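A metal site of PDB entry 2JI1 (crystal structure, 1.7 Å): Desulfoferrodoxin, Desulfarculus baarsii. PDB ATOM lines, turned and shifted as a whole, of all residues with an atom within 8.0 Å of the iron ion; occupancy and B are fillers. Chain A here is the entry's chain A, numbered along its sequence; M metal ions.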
ATOM      1  N   VAL A  42      18.016 -11.608   9.657  1.00  0.00           N
ATOM      2  CA  VAL A  42      18.401 -11.087  10.965  1.00  0.00           C
ATOM      3  C   VAL A  42      19.577 -11.835  11.582  1.00  0.00           C
ATOM      4  O   VAL A  42      19.738 -13.044  11.392  1.00  0.00           O
ATOM      5  CB  VAL A  42      17.196 -11.122  11.953  1.00  0.00           C
ATOM      6  CG1 VAL A  42      17.649 -10.753  13.359  1.00  0.00           C
ATOM      7  CG2 VAL A  42      16.131 -10.164  11.478  1.00  0.00           C
ATOM      8  N   ALA A  44      20.707 -13.530  14.234  1.00  0.00           N
ATOM      9  CA  ALA A  44      20.265 -14.237  15.426  1.00  0.00           C
ATOM     10  C   ALA A  44      20.724 -15.692  15.350  1.00  0.00           C
ATOM     11  O   ALA A  44      21.213 -16.146  14.321  1.00  0.00           O
ATOM     12  CB  ALA A  44      18.745 -14.175  15.522  1.00  0.00           C
ATOM     13  N   ALA A  45      20.567 -16.411  16.451  1.00  0.00           N
ATOM     14  CA  ALA A  45      20.974 -17.806  16.537  1.00  0.00           C
ATOM     15  C   ALA A  45      20.176 -18.665  15.567  1.00  0.00           C
ATOM     16  O   ALA A  45      18.971 -18.879  15.753  1.00  0.00           O
ATOM     17  CB  ALA A  45      20.811 -18.322  17.950  1.00  0.00           C
ATOM     18  N   LYS A  48      18.139 -21.711  16.773  1.00  0.00           N
ATOM     19  CA  LYS A  48      16.922 -21.430  17.523  1.00  0.00           C
ATOM     20  C   LYS A  48      15.834 -20.789  16.661  1.00  0.00           C
ATOM     21  O   LYS A  48      14.686 -20.693  17.096  1.00  0.00           O
ATOM     22  CB  LYS A  48      17.210 -20.496  18.699  1.00  0.00           C
ATOM     23  CG  LYS A  48      18.074 -21.107  19.784  1.00  0.00           C
ATOM     24  CD  LYS A  48      18.384 -20.073  20.866  1.00  0.00           C
ATOM     25  CE  LYS A  48      19.270 -20.660  21.943  1.00  0.00           C
ATOM     26  NZ  LYS A  48      19.625 -19.646  22.973  1.00  0.00           N
ATOM     27  N   HIS A  49      16.177 -20.353  15.457  1.00  0.00           N
ATOM     28  CA  HIS A  49      15.186 -19.705  14.603  1.00  0.00           C
ATOM     29  C   HIS A  49      14.823 -20.386  13.287  1.00  0.00           C
ATOM     30  O   HIS A  49      13.689 -20.257  12.825  1.00  0.00           O
ATOM     31  CB  HIS A  49      15.604 -18.254  14.316  1.00  0.00           C
ATOM     32  CG  HIS A  49      15.612 -17.386  15.544  1.00  0.00           C
ATOM     33  ND1 HIS A  49      16.719 -17.249  16.347  1.00  0.00           N
ATOM     34  CD2 HIS A  49      14.634 -16.630  16.102  1.00  0.00           C
ATOM     35  CE1 HIS A  49      16.425 -16.445  17.352  1.00  0.00           C
ATOM     36  NE2 HIS A  49      15.173 -16.059  17.229  1.00  0.00           N
ATOM     37  N   VAL A  64      10.752 -24.956  16.069  1.00  0.00           N
ATOM     38  CA  VAL A  64      11.625 -23.797  15.975  1.00  0.00           C
ATOM     39  C   VAL A  64      12.525 -23.727  17.207  1.00  0.00           C
ATOM     40  O   VAL A  64      12.059 -23.397  18.292  1.00  0.00           O
ATOM     41  CB  VAL A  64      10.776 -22.493  15.898  1.00  0.00           C
ATOM     42  CG1 VAL A  64      11.696 -21.290  15.773  1.00  0.00           C
ATOM     43  CG2 VAL A  64       9.803 -22.567  14.719  1.00  0.00           C
ATOM     44  N   HIS A  69      13.387 -22.760  20.748  1.00  0.00           N
ATOM     45  CA  HIS A  69      13.452 -21.314  20.921  1.00  0.00           C
ATOM     46  C   HIS A  69      12.655 -20.936  22.162  1.00  0.00           C
ATOM     47  O   HIS A  69      11.691 -21.606  22.529  1.00  0.00           O
ATOM     48  CB  HIS A  69      12.880 -20.619  19.679  1.00  0.00           C
ATOM     49  CG  HIS A  69      12.936 -19.121  19.750  1.00  0.00           C
ATOM     50  ND1 HIS A  69      12.075 -18.374  20.526  1.00  0.00           N
ATOM     51  CD2 HIS A  69      13.748 -18.239  19.129  1.00  0.00           C
ATOM     52  CE1 HIS A  69      12.361 -17.089  20.381  1.00  0.00           C
ATOM     53  NE2 HIS A  69      13.379 -16.982  19.539  1.00  0.00           N
ATOM     54  N   PRO A  70      13.060 -19.852  22.850  1.00  0.00           N
ATOM     55  CA  PRO A  70      12.328 -19.416  24.042  1.00  0.00           C
ATOM     56  C   PRO A  70      10.877 -19.090  23.724  1.00  0.00           C
ATOM     57  O   PRO A  70      10.544 -18.736  22.590  1.00  0.00           O
ATOM     58  CB  PRO A  70      13.103 -18.172  24.484  1.00  0.00           C
ATOM     59  CG  PRO A  70      14.501 -18.474  24.043  1.00  0.00           C
ATOM     60  CD  PRO A  70      14.292 -19.062  22.665  1.00  0.00           C
ATOM     61  N   LYS A  74       8.254 -11.730  26.792  1.00  0.00           N
ATOM     62  CA  LYS A  74       9.012 -10.745  25.996  1.00  0.00           C
ATOM     63  C   LYS A  74       9.749 -11.294  24.768  1.00  0.00           C
ATOM     64  O   LYS A  74      10.305 -10.553  23.941  1.00  0.00           O
ATOM     65  CB  LYS A  74      10.051 -10.012  26.883  1.00  0.00           C
ATOM     66  CG  LYS A  74       9.483  -8.884  27.680  1.00  0.00           C
ATOM     67  CD  LYS A  74      10.592  -7.907  28.072  1.00  0.00           C
ATOM     68  N   HIS A  75       9.770 -12.611  24.642  1.00  0.00           N
ATOM     69  CA  HIS A  75      10.486 -13.237  23.545  1.00  0.00           C
ATOM     70  C   HIS A  75       9.897 -14.606  23.215  1.00  0.00           C
ATOM     71  O   HIS A  75      10.100 -15.568  23.960  1.00  0.00           O
ATOM     72  CB  HIS A  75      11.969 -13.416  23.917  1.00  0.00           C
ATOM     73  CG  HIS A  75      12.829 -13.919  22.790  1.00  0.00           C
ATOM     74  ND1 HIS A  75      14.030 -14.577  23.004  1.00  0.00           N
ATOM     75  CD2 HIS A  75      12.685 -13.812  21.451  1.00  0.00           C
ATOM     76  CE1 HIS A  75      14.576 -14.853  21.831  1.00  0.00           C
ATOM     77  NE2 HIS A  75      13.791 -14.410  20.876  1.00  0.00           N
ATOM     78  N   TYR A  76       9.165 -14.689  22.117  1.00  0.00           N
ATOM     79  CA  TYR A  76       8.555 -15.952  21.717  1.00  0.00           C
ATOM     80  C   TYR A  76       8.239 -16.002  20.235  1.00  0.00           C
ATOM     81  O   TYR A  76       8.232 -14.970  19.552  1.00  0.00           O
ATOM     82  CB  TYR A  76       7.266 -16.191  22.514  1.00  0.00           C
ATOM     83  CG  TYR A  76       6.135 -15.214  22.202  1.00  0.00           C
ATOM     84  CD1 TYR A  76       6.193 -13.898  22.645  1.00  0.00           C
ATOM     85  CD2 TYR A  76       5.025 -15.619  21.476  1.00  0.00           C
ATOM     86  CE1 TYR A  76       5.161 -13.003  22.371  1.00  0.00           C
ATOM     87  CE2 TYR A  76       3.977 -14.739  21.190  1.00  0.00           C
ATOM     88  CZ  TYR A  76       4.059 -13.426  21.639  1.00  0.00           C
ATOM     89  OH  TYR A  76       3.025 -12.549  21.381  1.00  0.00           O
ATOM     90  N   ILE A  77       8.003 -17.210  19.741  1.00  0.00           N
ATOM     91  CA  ILE A  77       7.649 -17.411  18.344  1.00  0.00           C
ATOM     92  C   ILE A  77       6.157 -17.119  18.240  1.00  0.00           C
ATOM     93  O   ILE A  77       5.341 -17.817  18.825  1.00  0.00           O
ATOM     94  CB  ILE A  77       7.930 -18.877  17.919  1.00  0.00           C
ATOM     95  CG1 ILE A  77       9.408 -19.214  18.172  1.00  0.00           C
ATOM     96  CG2 ILE A  77       7.539 -19.080  16.447  1.00  0.00           C
ATOM     97  CD1 ILE A  77      10.397 -18.197  17.598  1.00  0.00           C
ATOM     98  N   GLU A 114       8.519 -19.128  10.259  1.00  0.00           N
ATOM     99  CA  GLU A 114       8.228 -18.783  11.642  1.00  0.00           C
ATOM    100  C   GLU A 114       8.594 -17.332  11.870  1.00  0.00           C
ATOM    101  O   GLU A 114       9.468 -16.782  11.190  1.00  0.00           O
ATOM    102  CB  GLU A 114       9.008 -19.692  12.608  1.00  0.00           C
ATOM    103  CG  GLU A 114      10.535 -19.511  12.621  1.00  0.00           C
ATOM    104  CD  GLU A 114      11.019 -18.460  13.616  1.00  0.00           C
ATOM    105  OE1 GLU A 114      10.173 -17.722  14.165  1.00  0.00           O
ATOM    106  OE2 GLU A 114      12.241 -18.364  13.837  1.00  0.00           O
ATOM    107  N   TYR A 115       7.909 -16.701  12.819  1.00  0.00           N
ATOM    108  CA  TYR A 115       8.199 -15.314  13.132  1.00  0.00           C
ATOM    109  C   TYR A 115       8.421 -15.137  14.621  1.00  0.00           C
ATOM    110  O   TYR A 115       7.574 -15.509  15.425  1.00  0.00           O
ATOM    111  CB  TYR A 115       7.064 -14.410  12.654  1.00  0.00           C
ATOM    112  CG  TYR A 115       7.388 -12.932  12.810  1.00  0.00           C
ATOM    113  CD1 TYR A 115       7.096 -12.252  13.983  1.00  0.00           C
ATOM    114  CD2 TYR A 115       8.035 -12.244  11.786  1.00  0.00           C
ATOM    115  CE1 TYR A 115       7.447 -10.916  14.152  1.00  0.00           C
ATOM    116  CE2 TYR A 115       8.397 -10.911  11.946  1.00  0.00           C
ATOM    117  CZ  TYR A 115       8.096 -10.250  13.128  1.00  0.00           C
ATOM    118  OH  TYR A 115       8.496  -8.936  13.295  1.00  0.00           O
ATOM    119  N   CYS A 116       9.576 -14.587  14.977  1.00  0.00           N
ATOM    120  CA  CYS A 116       9.930 -14.328  16.371  1.00  0.00           C
ATOM    121  C   CYS A 116       9.680 -12.834  16.618  1.00  0.00           C
ATOM    122  O   CYS A 116      10.106 -12.009  15.807  1.00  0.00           O
ATOM    123  CB  CYS A 116      11.401 -14.666  16.617  1.00  0.00           C
ATOM    124  SG  CYS A 116      12.044 -14.075  18.172  1.00  0.00           S
ATOM    125  N   ASN A 117       8.999 -12.488  17.705  1.00  0.00           N
ATOM    126  CA  ASN A 117       8.687 -11.084  17.962  1.00  0.00           C
ATOM    127  C   ASN A 117       9.934 -10.202  18.038  1.00  0.00           C
ATOM    128  O   ASN A 117       9.872  -8.992  17.779  1.00  0.00           O
ATOM    129  CB  ASN A 117       7.879 -10.935  19.255  1.00  0.00           C
ATOM    130  CG  ASN A 117       8.698 -11.172  20.499  1.00  0.00           C
ATOM    131  OD1 ASN A 117       9.337 -12.218  20.651  1.00  0.00           O
ATOM    132  ND2 ASN A 117       8.693 -10.203  21.411  1.00  0.00           N
ATOM    133  N   ILE A 118      11.070 -10.792  18.372  1.00  0.00           N
ATOM    134  CA  ILE A 118      12.300 -10.037  18.459  1.00  0.00           C
ATOM    135  C   ILE A 118      13.208 -10.227  17.254  1.00  0.00           C
ATOM    136  O   ILE A 118      13.709  -9.260  16.674  1.00  0.00           O
ATOM    137  CB  ILE A 118      13.126 -10.407  19.734  1.00  0.00           C
ATOM    138  CG1 ILE A 118      12.312 -10.124  20.996  1.00  0.00           C
ATOM    139  CG2 ILE A 118      14.436  -9.637  19.749  1.00  0.00           C
ATOM    140  CD1 ILE A 118      11.843  -8.683  21.134  1.00  0.00           C
ATOM    141  N   HIS A 119      13.413 -11.483  16.855  1.00  0.00           N
ATOM    142  CA  HIS A 119      14.328 -11.776  15.758  1.00  0.00           C
ATOM    143  C   HIS A 119      13.807 -11.944  14.345  1.00  0.00           C
ATOM    144  O   HIS A 119      14.516 -12.412  13.456  1.00  0.00           O
ATOM    145  CB  HIS A 119      15.181 -12.979  16.158  1.00  0.00           C
ATOM    146  CG  HIS A 119      15.883 -12.807  17.464  1.00  0.00           C
ATOM    147  ND1 HIS A 119      15.496 -13.453  18.616  1.00  0.00           N
ATOM    148  CD2 HIS A 119      16.911 -11.993  17.820  1.00  0.00           C
ATOM    149  CE1 HIS A 119      16.249 -13.064  19.620  1.00  0.00           C
ATOM    150  NE2 HIS A 119      17.117 -12.177  19.162  1.00  0.00           N
ATOM    151  N   GLY A 120      12.561 -11.544  14.122  1.00  0.00           N
ATOM    152  CA  GLY A 120      12.021 -11.592  12.771  1.00  0.00           C
ATOM    153  C   GLY A 120      11.579 -12.893  12.133  1.00  0.00           C
ATOM    154  O   GLY A 120      11.313 -13.896  12.800  1.00  0.00           O
ATOM    155  N   TRP A 122      11.819 -16.190   9.601  1.00  0.00           N
ATOM    156  CA  TRP A 122      12.746 -17.258   9.218  1.00  0.00           C
ATOM    157  C   TRP A 122      12.024 -18.357   8.450  1.00  0.00           C
ATOM    158  O   TRP A 122      10.826 -18.562   8.617  1.00  0.00           O
ATOM    159  CB  TRP A 122      13.404 -17.848  10.470  1.00  0.00           C
ATOM    160  CG  TRP A 122      14.264 -16.861  11.176  1.00  0.00           C
ATOM    161  CD1 TRP A 122      13.843 -15.825  11.969  1.00  0.00           C
ATOM    162  CD2 TRP A 122      15.688 -16.733  11.069  1.00  0.00           C
ATOM    163  NE1 TRP A 122      14.928 -15.060  12.345  1.00  0.00           N
ATOM    164  CE2 TRP A 122      16.066 -15.597  11.804  1.00  0.00           C
ATOM    165  CE3 TRP A 122      16.672 -17.475  10.412  1.00  0.00           C
ATOM    166  CZ2 TRP A 122      17.394 -15.171  11.908  1.00  0.00           C
ATOM    167  CZ3 TRP A 122      18.004 -17.057  10.513  1.00  0.00           C
ATOM    168  CH2 TRP A 122      18.348 -15.915  11.250  1.00  0.00           C
HETATM  169 FE    FE M   1      14.143 -15.054  18.858  1.00  0.00          FE
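The backbone carbonyl oxygen (O) of His 119 is in hydrogen-bond range of the indole nitrogen (NE1) of Trp 122 (2.9 Å).
The backbone carbonyl oxygen (O) of His 49 lies close to the side-chain carboxylate (OE2) of Glu 114, at 2.6 Å.
A ring nitrogen (ND1) of His 49 sits at hydrogen-bond distance from the backbone carbonyl oxygen (O) of Ala 45, 2.8 Å away.
N of His 69 lies within hydrogen-bond range of O of Val 64.
The side-chain sulfur (SG) of Cys 116 sits close to the backbone NH (N) of Ile 118, at 3.4 Å.
N of Cys 116 lies within hydrogen-bond range of OE1 of Glu 114 (3.3 Å).
The iron ion is bound by ND1 of His 119 (2.1 Å), NE2 of His 75 (2.1 Å), NE2 of His 49 (2.2 Å), NE2 of His 69 (2.2 Å) and SG of Cys 116 (2.4 Å).
The iron ion has five donor atoms within binding distance.
Of the 20 residues printed, 5 come within 4 Å of the iron ion.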
